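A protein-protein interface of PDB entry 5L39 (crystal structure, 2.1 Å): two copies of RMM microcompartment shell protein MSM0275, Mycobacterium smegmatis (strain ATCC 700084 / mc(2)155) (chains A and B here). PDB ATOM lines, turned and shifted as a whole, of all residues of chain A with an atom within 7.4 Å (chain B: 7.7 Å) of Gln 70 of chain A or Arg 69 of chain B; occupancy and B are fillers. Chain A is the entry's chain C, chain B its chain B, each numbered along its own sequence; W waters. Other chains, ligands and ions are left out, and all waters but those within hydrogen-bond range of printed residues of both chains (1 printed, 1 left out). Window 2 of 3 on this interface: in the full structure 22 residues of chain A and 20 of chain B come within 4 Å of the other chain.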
ATOM      1  N   ARG A   5      14.251 -24.940 -24.220  1.00  0.00           N
ATOM      2  CA  ARG A   5      13.189 -25.350 -23.302  1.00  0.00           C
ATOM      3  C   ARG A   5      11.842 -24.749 -23.681  1.00  0.00           C
ATOM      4  O   ARG A   5      10.795 -25.331 -23.387  1.00  0.00           O
ATOM      5  CB  ARG A   5      13.562 -24.988 -21.868  1.00  0.00           C
ATOM      6  CG  ARG A   5      14.769 -25.776 -21.363  1.00  0.00           C
ATOM      7  CD  ARG A   5      15.194 -25.364 -19.955  1.00  0.00           C
ATOM      8  NE  ARG A   5      14.137 -25.544 -18.961  1.00  0.00           N
ATOM      9  CZ  ARG A   5      13.787 -26.717 -18.435  1.00  0.00           C
ATOM     10  NH1 ARG A   5      14.399 -27.829 -18.817  1.00  0.00           N
ATOM     11  NH2 ARG A   5      12.814 -26.778 -17.528  1.00  0.00           N
ATOM     12  N   GLU A  40      13.276 -19.825 -23.544  1.00  0.00           N
ATOM     13  CA  GLU A  40      13.949 -20.359 -22.362  1.00  0.00           C
ATOM     14  C   GLU A  40      14.984 -21.387 -22.794  1.00  0.00           C
ATOM     15  O   GLU A  40      14.699 -22.236 -23.636  1.00  0.00           O
ATOM     16  CB  GLU A  40      12.952 -20.993 -21.380  1.00  0.00           C
ATOM     17  CG  GLU A  40      13.631 -21.560 -20.119  1.00  0.00           C
ATOM     18  CD  GLU A  40      12.671 -22.249 -19.150  1.00  0.00           C
ATOM     19  OE1 GLU A  40      11.438 -22.187 -19.371  1.00  0.00           O
ATOM     20  OE2 GLU A  40      13.158 -22.847 -18.159  1.00  0.00           O
ATOM     21  N   VAL A  41      16.192 -21.307 -22.243  1.00  0.00           N
ATOM     22  CA  VAL A  41      17.242 -22.235 -22.657  1.00  0.00           C
ATOM     23  C   VAL A  41      18.075 -22.786 -21.499  1.00  0.00           C
ATOM     24  O   VAL A  41      18.057 -22.253 -20.386  1.00  0.00           O
ATOM     25  CB  VAL A  41      18.214 -21.575 -23.669  1.00  0.00           C
ATOM     26  CG1 VAL A  41      17.465 -21.078 -24.911  1.00  0.00           C
ATOM     27  CG2 VAL A  41      18.999 -20.444 -23.006  1.00  0.00           C
ATOM     28  N   ALA A  42      18.792 -23.867 -21.788  1.00  0.00           N
ATOM     29  CA  ALA A  42      19.849 -24.381 -20.927  1.00  0.00           C
ATOM     30  C   ALA A  42      21.060 -24.667 -21.809  1.00  0.00           C
ATOM     31  O   ALA A  42      20.896 -25.122 -22.941  1.00  0.00           O
ATOM     32  CB  ALA A  42      19.407 -25.642 -20.185  1.00  0.00           C
ATOM     33  N   PRO A  43      22.276 -24.378 -21.313  1.00  0.00           N
ATOM     34  CA  PRO A  43      22.563 -23.745 -20.020  1.00  0.00           C
ATOM     35  C   PRO A  43      22.151 -22.276 -20.041  1.00  0.00           C
ATOM     36  O   PRO A  43      22.106 -21.678 -21.124  1.00  0.00           O
ATOM     37  CB  PRO A  43      24.080 -23.901 -19.878  1.00  0.00           C
ATOM     38  CG  PRO A  43      24.574 -23.921 -21.295  1.00  0.00           C
ATOM     39  CD  PRO A  43      23.502 -24.618 -22.096  1.00  0.00           C
ATOM     40  N   GLY A  44      21.844 -21.718 -18.872  1.00  0.00           N
ATOM     41  CA  GLY A  44      21.226 -20.405 -18.770  1.00  0.00           C
ATOM     42  C   GLY A  44      21.907 -19.258 -19.503  1.00  0.00           C
ATOM     43  O   GLY A  44      21.234 -18.394 -20.061  1.00  0.00           O
ATOM     44  N   LEU A  45      23.235 -19.244 -19.508  1.00  0.00           N
ATOM     45  CA  LEU A  45      23.979 -18.117 -20.065  1.00  0.00           C
ATOM     46  C   LEU A  45      23.912 -18.061 -21.587  1.00  0.00           C
ATOM     47  O   LEU A  45      24.289 -17.057 -22.188  1.00  0.00           O
ATOM     48  CB  LEU A  45      25.443 -18.160 -19.624  1.00  0.00           C
ATOM     49  CG  LEU A  45      25.936 -16.878 -18.953  1.00  0.00           C
ATOM     50  CD1 LEU A  45      25.186 -16.638 -17.655  1.00  0.00           C
ATOM     51  CD2 LEU A  45      27.417 -16.949 -18.690  1.00  0.00           C
ATOM     52  N   VAL A  67      18.871 -14.821 -16.023  1.00  0.00           N
ATOM     53  CA  VAL A  67      19.504 -16.123 -15.861  1.00  0.00           C
ATOM     54  C   VAL A  67      19.342 -16.559 -14.409  1.00  0.00           C
ATOM     55  O   VAL A  67      19.929 -15.966 -13.505  1.00  0.00           O
ATOM     56  CB  VAL A  67      21.001 -16.110 -16.229  1.00  0.00           C
ATOM     57  CG1 VAL A  67      21.537 -17.532 -16.278  1.00  0.00           C
ATOM     58  CG2 VAL A  67      21.237 -15.413 -17.561  1.00  0.00           C
ATOM     59  N   GLU A  68      18.537 -17.592 -14.181  1.00  0.00           N
ATOM     60  CA  GLU A  68      18.290 -18.056 -12.815  1.00  0.00           C
ATOM     61  C   GLU A  68      19.216 -19.212 -12.473  1.00  0.00           C
ATOM     62  O   GLU A  68      20.275 -19.347 -13.077  1.00  0.00           O
ATOM     63  CB  GLU A  68      16.814 -18.446 -12.642  1.00  0.00           C
ATOM     64  CG  GLU A  68      16.369 -19.637 -13.488  1.00  0.00           C
ATOM     65  CD  GLU A  68      16.193 -20.895 -12.666  1.00  0.00           C
ATOM     66  OE1 GLU A  68      16.543 -21.972 -13.165  1.00  0.00           O
ATOM     67  OE2 GLU A  68      15.689 -20.793 -11.538  1.00  0.00           O
ATOM     68  N   ARG A  69      18.824 -20.035 -11.505  1.00  0.00           N
ATOM     69  CA  ARG A  69      19.689 -21.106 -11.013  1.00  0.00           C
ATOM     70  C   ARG A  69      20.223 -21.994 -12.136  1.00  0.00           C
ATOM     71  O   ARG A  69      21.406 -22.317 -12.170  1.00  0.00           O
ATOM     72  CB  ARG A  69      18.950 -21.985  -9.987  1.00  0.00           C
ATOM     73  CG  ARG A  69      19.844 -23.079  -9.406  1.00  0.00           C
ATOM     74  CD  ARG A  69      19.189 -23.901  -8.286  1.00  0.00           C
ATOM     75  NE  ARG A  69      20.136 -24.870  -7.728  1.00  0.00           N
ATOM     76  CZ  ARG A  69      21.033 -24.588  -6.784  1.00  0.00           C
ATOM     77  NH1 ARG A  69      21.112 -23.365  -6.273  1.00  0.00           N
ATOM     78  NH2 ARG A  69      21.853 -25.532  -6.345  1.00  0.00           N
ATOM     79  N   GLN A  70      19.347 -22.380 -13.056  1.00  0.00           N
ATOM     80  CA  GLN A  70      19.729 -23.264 -14.149  1.00  0.00           C
ATOM     81  C   GLN A  70      19.461 -22.641 -15.516  1.00  0.00           C
ATOM     82  O   GLN A  70      20.272 -22.768 -16.430  1.00  0.00           O
ATOM     83  CB  GLN A  70      18.975 -24.592 -14.055  1.00  0.00           C
ATOM     84  CG  GLN A  70      19.196 -25.370 -12.768  1.00  0.00           C
ATOM     85  CD  GLN A  70      18.433 -26.677 -12.763  1.00  0.00           C
ATOM     86  OE1 GLN A  70      17.312 -26.763 -12.245  1.00  0.00           O
ATOM     87  NE2 GLN A  70      19.025 -27.703 -13.360  1.00  0.00           N
ATOM     88  N   PHE A  71      18.320 -21.973 -15.653  1.00  0.00           N
ATOM     89  CA  PHE A  71      17.800 -21.643 -16.977  1.00  0.00           C
ATOM     90  C   PHE A  71      17.871 -20.156 -17.324  1.00  0.00           C
ATOM     91  O   PHE A  71      17.893 -19.292 -16.445  1.00  0.00           O
ATOM     92  CB  PHE A  71      16.363 -22.145 -17.082  1.00  0.00           C
ATOM     93  CG  PHE A  71      16.203 -23.586 -16.674  1.00  0.00           C
ATOM     94  CD1 PHE A  71      17.040 -24.561 -17.195  1.00  0.00           C
ATOM     95  CD2 PHE A  71      15.245 -23.960 -15.743  1.00  0.00           C
ATOM     96  CE1 PHE A  71      16.902 -25.890 -16.822  1.00  0.00           C
ATOM     97  CE2 PHE A  71      15.101 -25.292 -15.363  1.00  0.00           C
ATOM     98  CZ  PHE A  71      15.930 -26.256 -15.900  1.00  0.00           C
ATOM     99  N   GLY A  72      17.913 -19.871 -18.623  1.00  0.00           N
ATOM    100  CA  GLY A  72      17.988 -18.508 -19.115  1.00  0.00           C
ATOM    101  C   GLY A  72      16.711 -18.123 -19.840  1.00  0.00           C
ATOM    102  O   GLY A  72      16.119 -18.939 -20.545  1.00  0.00           O
ATOM    103  N   TYR A  73      16.284 -16.879 -19.665  1.00  0.00           N
ATOM    104  CA  TYR A  73      14.996 -16.436 -20.184  1.00  0.00           C
ATOM    105  C   TYR A  73      15.106 -15.130 -20.945  1.00  0.00           C
ATOM    106  O   TYR A  73      15.736 -14.187 -20.475  1.00  0.00           O
ATOM    107  CB  TYR A  73      13.987 -16.259 -19.050  1.00  0.00           C
ATOM    108  CG  TYR A  73      13.734 -17.505 -18.241  1.00  0.00           C
ATOM    109  CD1 TYR A  73      14.649 -17.939 -17.292  1.00  0.00           C
ATOM    110  CD2 TYR A  73      12.576 -18.242 -18.421  1.00  0.00           C
ATOM    111  CE1 TYR A  73      14.419 -19.080 -16.540  1.00  0.00           C
ATOM    112  CE2 TYR A  73      12.334 -19.378 -17.673  1.00  0.00           C
ATOM    113  CZ  TYR A  73      13.259 -19.795 -16.736  1.00  0.00           C
ATOM    114  OH  TYR A  73      13.019 -20.931 -16.006  1.00  0.00           O
ATOM    115  N   GLU A 142       0.489 -25.711 -12.536  1.00  0.00           N
ATOM    116  CA  GLU A 142       1.944 -25.766 -12.510  1.00  0.00           C
ATOM    117  C   GLU A 142       2.428 -26.433 -13.792  1.00  0.00           C
ATOM    118  O   GLU A 142       1.896 -27.461 -14.189  1.00  0.00           O
ATOM    119  CB  GLU A 142       2.450 -26.522 -11.266  1.00  0.00           C
ATOM    120  CG  GLU A 142       3.966 -26.459 -11.065  1.00  0.00           C
ATOM    121  CD  GLU A 142       4.443 -27.080  -9.740  1.00  0.00           C
ATOM    122  OE1 GLU A 142       3.688 -27.856  -9.111  1.00  0.00           O
ATOM    123  OE2 GLU A 142       5.587 -26.788  -9.332  1.00  0.00           O
ATOM    124  N   ILE A 170       9.486 -18.307 -14.231  1.00  0.00           N
ATOM    125  CA  ILE A 170      10.927 -18.467 -14.138  1.00  0.00           C
ATOM    126  C   ILE A 170      11.262 -19.433 -13.011  1.00  0.00           C
ATOM    127  O   ILE A 170      10.820 -19.249 -11.883  1.00  0.00           O
ATOM    128  CB  ILE A 170      11.607 -17.112 -13.906  1.00  0.00           C
ATOM    129  CG1 ILE A 170      11.526 -16.277 -15.188  1.00  0.00           C
ATOM    130  CG2 ILE A 170      13.068 -17.287 -13.438  1.00  0.00           C
ATOM    131  CD1 ILE A 170      11.817 -14.819 -14.988  1.00  0.00           C
ATOM    132  N   GLY A 171      12.025 -20.477 -13.321  1.00  0.00           N
ATOM    133  CA  GLY A 171      12.393 -21.465 -12.321  1.00  0.00           C
ATOM    134  C   GLY A 171      12.321 -22.867 -12.889  1.00  0.00           C
ATOM    135  O   GLY A 171      12.312 -23.052 -14.110  1.00  0.00           O
ATOM    136  N   ALA A 172      12.276 -23.862 -12.010  1.00  0.00           N
ATOM    137  CA  ALA A 172      12.138 -25.243 -12.455  1.00  0.00           C
ATOM    138  C   ALA A 172      10.722 -25.495 -12.954  1.00  0.00           C
ATOM    139  O   ALA A 172      10.510 -26.271 -13.889  1.00  0.00           O
ATOM    140  CB  ALA A 172      12.486 -26.211 -11.334  1.00  0.00           C
ATOM    141  N   THR A 173       9.755 -24.839 -12.321  1.00  0.00           N
ATOM    142  CA  THR A 173       8.355 -24.947 -12.714  1.00  0.00           C
ATOM    143  C   THR A 173       7.705 -23.567 -12.751  1.00  0.00           C
ATOM    144  O   THR A 173       8.156 -22.647 -12.072  1.00  0.00           O
ATOM    145  CB  THR A 173       7.553 -25.846 -11.758  1.00  0.00           C
ATOM    146  OG1 THR A 173       7.397 -25.187 -10.495  1.00  0.00           O
ATOM    147  CG2 THR A 173       8.248 -27.186 -11.554  1.00  0.00           C
ATOM    148  N   GLY A 174       6.663 -23.422 -13.566  1.00  0.00           N
ATOM    149  CA  GLY A 174       5.916 -22.178 -13.640  1.00  0.00           C
ATOM    150  C   GLY A 174       4.580 -22.350 -12.943  1.00  0.00           C
ATOM    151  O   GLY A 174       4.091 -23.474 -12.815  1.00  0.00           O
ATOM    152  N   ARG A 175       3.992 -21.252 -12.476  1.00  0.00           N
ATOM    153  CA  ARG A 175       2.764 -21.334 -11.685  1.00  0.00           C
ATOM    154  C   ARG A 175       1.804 -20.200 -11.990  1.00  0.00           C
ATOM    155  O   ARG A 175       2.214 -19.066 -12.252  1.00  0.00           O
ATOM    156  CB  ARG A 175       3.079 -21.333 -10.187  1.00  0.00           C
ATOM    157  CG  ARG A 175       3.941 -22.493  -9.736  1.00  0.00           C
ATOM    158  CD  ARG A 175       5.048 -22.033  -8.821  1.00  0.00           C
ATOM    159  NE  ARG A 175       6.145 -22.994  -8.808  1.00  0.00           N
ATOM    160  CZ  ARG A 175       7.144 -22.973  -7.934  1.00  0.00           C
ATOM    161  NH1 ARG A 175       7.180 -22.042  -6.990  1.00  0.00           N
ATOM    162  NH2 ARG A 175       8.102 -23.887  -8.005  1.00  0.00           N
ATOM    163  N   GLY B  44       5.144 -29.324  -6.235  1.00  0.00           N
ATOM    164  CA  GLY B  44       4.839 -28.364  -5.191  1.00  0.00           C
ATOM    165  C   GLY B  44       3.399 -27.882  -5.151  1.00  0.00           C
ATOM    166  O   GLY B  44       2.807 -27.793  -4.072  1.00  0.00           O
ATOM    167  N   VAL B  66       3.920 -23.035   1.533  1.00  0.00           N
ATOM    168  CA  VAL B  66       5.042 -22.651   0.679  1.00  0.00           C
ATOM    169  C   VAL B  66       5.167 -23.554  -0.534  1.00  0.00           C
ATOM    170  O   VAL B  66       5.197 -24.779  -0.409  1.00  0.00           O
ATOM    171  CB  VAL B  66       6.397 -22.685   1.445  1.00  0.00           C
ATOM    172  CG1 VAL B  66       7.563 -22.461   0.478  1.00  0.00           C
ATOM    173  CG2 VAL B  66       6.425 -21.642   2.543  1.00  0.00           C
ATOM    174  N   VAL B  67       5.231 -22.937  -1.709  1.00  0.00           N
ATOM    175  CA  VAL B  67       5.628 -23.631  -2.925  1.00  0.00           C
ATOM    176  C   VAL B  67       6.990 -23.086  -3.349  1.00  0.00           C
ATOM    177  O   VAL B  67       7.079 -22.010  -3.939  1.00  0.00           O
ATOM    178  CB  VAL B  67       4.604 -23.453  -4.062  1.00  0.00           C
ATOM    179  CG1 VAL B  67       4.922 -24.403  -5.204  1.00  0.00           C
ATOM    180  CG2 VAL B  67       3.183 -23.683  -3.562  1.00  0.00           C
ATOM    181  N   GLU B  68       8.051 -23.823  -3.027  1.00  0.00           N
ATOM    182  CA  GLU B  68       9.408 -23.400  -3.370  1.00  0.00           C
ATOM    183  C   GLU B  68       9.780 -23.934  -4.749  1.00  0.00           C
ATOM    184  O   GLU B  68       8.893 -24.201  -5.558  1.00  0.00           O
ATOM    185  CB  GLU B  68      10.412 -23.853  -2.281  1.00  0.00           C
ATOM    186  CG  GLU B  68      10.592 -25.369  -2.143  1.00  0.00           C
ATOM    187  CD  GLU B  68      11.905 -25.864  -2.723  1.00  0.00           C
ATOM    188  OE1 GLU B  68      11.920 -26.982  -3.258  1.00  0.00           O
ATOM    189  OE2 GLU B  68      12.911 -25.141  -2.620  1.00  0.00           O
ATOM    190  N   ARG B  69      11.074 -24.094  -5.014  1.00  0.00           N
ATOM    191  CA  ARG B  69      11.526 -24.429  -6.366  1.00  0.00           C
ATOM    192  C   ARG B  69      10.916 -25.727  -6.887  1.00  0.00           C
ATOM    193  O   ARG B  69      10.453 -25.783  -8.023  1.00  0.00           O
ATOM    194  CB  ARG B  69      13.055 -24.530  -6.432  1.00  0.00           C
ATOM    195  CG  ARG B  69      13.582 -24.780  -7.853  1.00  0.00           C
ATOM    196  CD  ARG B  69      15.114 -24.832  -7.937  1.00  0.00           C
ATOM    197  NE  ARG B  69      15.550 -25.024  -9.318  1.00  0.00           N
ATOM    198  CZ  ARG B  69      15.702 -24.036 -10.192  1.00  0.00           C
ATOM    199  NH1 ARG B  69      16.086 -24.297 -11.434  1.00  0.00           N
ATOM    200  NH2 ARG B  69      15.466 -22.785  -9.820  1.00  0.00           N
ATOM    201  N   GLN B  70      10.913 -26.761  -6.052  1.00  0.00           N
ATOM    202  CA  GLN B  70      10.427 -28.074  -6.459  1.00  0.00           C
ATOM    203  C   GLN B  70       9.223 -28.521  -5.640  1.00  0.00           C
ATOM    204  O   GLN B  70       8.295 -29.123  -6.171  1.00  0.00           O
ATOM    205  CB  GLN B  70      11.522 -29.136  -6.315  1.00  0.00           C
ATOM    206  CG  GLN B  70      12.768 -28.943  -7.154  1.00  0.00           C
ATOM    207  CD  GLN B  70      13.807 -30.017  -6.866  1.00  0.00           C
ATOM    208  OE1 GLN B  70      14.614 -29.894  -5.936  1.00  0.00           O
ATOM    209  NE2 GLN B  70      13.779 -31.087  -7.651  1.00  0.00           N
ATOM    210  N   PHE B  71       9.249 -28.240  -4.341  1.00  0.00           N
ATOM    211  CA  PHE B  71       8.330 -28.895  -3.418  1.00  0.00           C
ATOM    212  C   PHE B  71       7.341 -27.934  -2.777  1.00  0.00           C
ATOM    213  O   PHE B  71       7.545 -26.717  -2.772  1.00  0.00           O
ATOM    214  CB  PHE B  71       9.130 -29.629  -2.335  1.00  0.00           C
ATOM    215  CG  PHE B  71      10.237 -30.475  -2.889  1.00  0.00           C
ATOM    216  CD1 PHE B  71       9.975 -31.413  -3.877  1.00  0.00           C
ATOM    217  CD2 PHE B  71      11.546 -30.305  -2.456  1.00  0.00           C
ATOM    218  CE1 PHE B  71      10.995 -32.188  -4.410  1.00  0.00           C
ATOM    219  CE2 PHE B  71      12.572 -31.074  -2.986  1.00  0.00           C
ATOM    220  CZ  PHE B  71      12.298 -32.017  -3.961  1.00  0.00           C
ATOM    221  N   GLY B  72       6.261 -28.499  -2.243  1.00  0.00           N
ATOM    222  CA  GLY B  72       5.237 -27.722  -1.571  1.00  0.00           C
ATOM    223  C   GLY B  72       5.095 -28.151  -0.126  1.00  0.00           C
ATOM    224  O   GLY B  72       5.226 -29.332   0.193  1.00  0.00           O
ATOM    225  N   TYR B  73       4.826 -27.189   0.750  1.00  0.00           N
ATOM    226  CA  TYR B  73       4.813 -27.440   2.187  1.00  0.00           C
ATOM    227  C   TYR B  73       3.550 -26.899   2.821  1.00  0.00           C
ATOM    228  O   TYR B  73       3.105 -25.799   2.493  1.00  0.00           O
ATOM    229  CB  TYR B  73       6.027 -26.795   2.858  1.00  0.00           C
ATOM    230  CG  TYR B  73       7.352 -27.273   2.324  1.00  0.00           C
ATOM    231  CD1 TYR B  73       7.851 -26.801   1.117  1.00  0.00           C
ATOM    232  CD2 TYR B  73       8.117 -28.182   3.041  1.00  0.00           C
ATOM    233  CE1 TYR B  73       9.078 -27.239   0.629  1.00  0.00           C
ATOM    234  CE2 TYR B  73       9.339 -28.618   2.564  1.00  0.00           C
ATOM    235  CZ  TYR B  73       9.811 -28.148   1.359  1.00  0.00           C
ATOM    236  OH  TYR B  73      11.027 -28.593   0.889  1.00  0.00           O
ATOM    237  N   ILE B 170      12.617 -26.287   4.578  1.00  0.00           N
ATOM    238  CA  ILE B 170      12.123 -26.100   3.221  1.00  0.00           C
ATOM    239  C   ILE B 170      13.297 -26.061   2.252  1.00  0.00           C
ATOM    240  O   ILE B 170      14.243 -25.307   2.450  1.00  0.00           O
ATOM    241  CB  ILE B 170      11.286 -24.810   3.107  1.00  0.00           C
ATOM    242  CG1 ILE B 170       9.949 -24.997   3.838  1.00  0.00           C
ATOM    243  CG2 ILE B 170      11.095 -24.404   1.632  1.00  0.00           C
ATOM    244  CD1 ILE B 170       9.081 -23.760   3.878  1.00  0.00           C
ATOM    245  N   GLY B 171      13.237 -26.894   1.219  1.00  0.00           N
ATOM    246  CA  GLY B 171      14.264 -26.903   0.194  1.00  0.00           C
ATOM    247  C   GLY B 171      14.556 -28.303  -0.301  1.00  0.00           C
ATOM    248  O   GLY B 171      13.751 -29.220  -0.129  1.00  0.00           O
ATOM    249  N   ALA B 172      15.715 -28.471  -0.925  1.00  0.00           N
ATOM    250  CA  ALA B 172      16.158 -29.793  -1.334  1.00  0.00           C
ATOM    251  C   ALA B 172      16.566 -30.611  -0.107  1.00  0.00           C
ATOM    252  O   ALA B 172      16.353 -31.820  -0.060  1.00  0.00           O
ATOM    253  CB  ALA B 172      17.311 -29.688  -2.318  1.00  0.00           C
HETATM  254  O   HOH W   1       6.989 -29.007  -8.700  1.00  0.00           O
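The guanidinium group (NH2) of Arg 69 of chain B is in salt-bridge range of the side-chain carboxylate (OE2) of Glu 68 of chain A (2.6 Å). NH2 of Arg 175 of chain A sits at hydrogen-bond distance from O of Glu 68 of chain B (2.6 Å). The guanidinium group (NH1) of Arg 69 of chain B is in hydrogen-bond range of the side-chain amide oxygen (OE1) of Gln 70 of chain A, 2.9 Å away. O of Val 67 of chain B sits at hydrogen-bond distance from NH1 of Arg 175 of chain A. The guanidinium group (NH2) of Arg 175 of chain A is in hydrogen-bond range of the backbone carbonyl oxygen (O) of Arg 69 of chain B.
The side-chain carboxylate (OE2) of Glu 142 of chain A sits at hydrogen-bond distance from the side-chain hydroxyl (OG1) of Thr 173 of chain A (2.7 Å). The side-chain carboxylate of Glu 142 of chain A is in salt-bridge range of the guanidinium group of Arg 175 of chain A (3.9 Å). NH2 of Arg 175 of chain A lies within hydrogen-bond range of OG1 of Thr 173 of chain A (2.9 Å). The side-chain carboxylate of Glu 68 of chain A lies within hydrogen-bond range of the backbone NH of Phe 71 of chain A. The side-chain carboxylate (OE1) of Glu 68 of chain B lies within hydrogen-bond range of the backbone NH (N) of Phe 71 of chain B (3.1 Å). The backbone carbonyl oxygen (O) of Gln 70 of chain B is in hydrogen-bond range of the backbone NH (N) of Gly 44 of chain B.
Among the printed residues, pairs that only touch across the chains: Glu 142 of chain A with Gly 44 of chain B (3.5 Å), Arg 69 of chain A with Arg 69 of chain B (3.6 Å), Ala 172 of chain A with Arg 69 of chain B (3.9 Å) and Thr 173 of chain A with Arg 69 of chain B (3.98 Å).
Gln 70 of chain A touches one residue of chain B. Arg 69 of chain B touches just these residues of chain A: Glu 68, Arg 69, Gln 70, Ala 172, Thr 173 and Arg 175. Of the printed residues of chain A, Val 67 of chain B touches Arg 175 (3.1 Å). Of the printed residues of chain B, Glu 142 of chain A touches Gly 44. Of the printed residues of chain B, Thr 173 of chain A touches Arg 69 (3.98 Å). Printed residues of chain B within 4 Å of Arg 175 of chain A: Val 67 (3.1 Å), Glu 68 (2.6 Å) and Arg 69 (3.0 Å). The nearest residue of chain B that does not touch Gln 70 of chain A is Gln 70 of chain B (7.2 Å). The nearest printed residue of chain A that does not touch Arg 69 of chain B is Phe 71 of chain A (4.2 Å).
Printed residues of chain B that touch a printed residue of chain A: Gly 44, Val 67, Glu 68 and Arg 69. Along chain B the printed residues that touch a printed residue of chain A span positions 44 to 69. Among the printed residues, 9 pairs touch across the chains.
Glu 68 of chain A touches Arg 69 of chain B, but with the chains exchanged Arg 69 of chain A does not touch Glu 68 of chain B (8.5 Å). Arg 69 of chain B touches its own counterpart, Arg 69 of chain A. Gln 70 of chain A touches Arg 69 of chain B, but with the chains exchanged Arg 69 of chain A does not touch Gln 70 of chain B (7.7 Å). Ala 172 of chain A touches Arg 69 of chain B, but with the chains exchanged Arg 69 of chain A does not touch Ala 172 of chain B (7.4 Å). Of the 9 pairs that touch across the chains among the printed residues, 1 has its exchanged pair printed and touching as well.
Water W1 lies within hydrogen-bond range of OE2 of Glu 142 of chain A, O of Gln 70 of chain B and N of Gly 44 of chain B.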
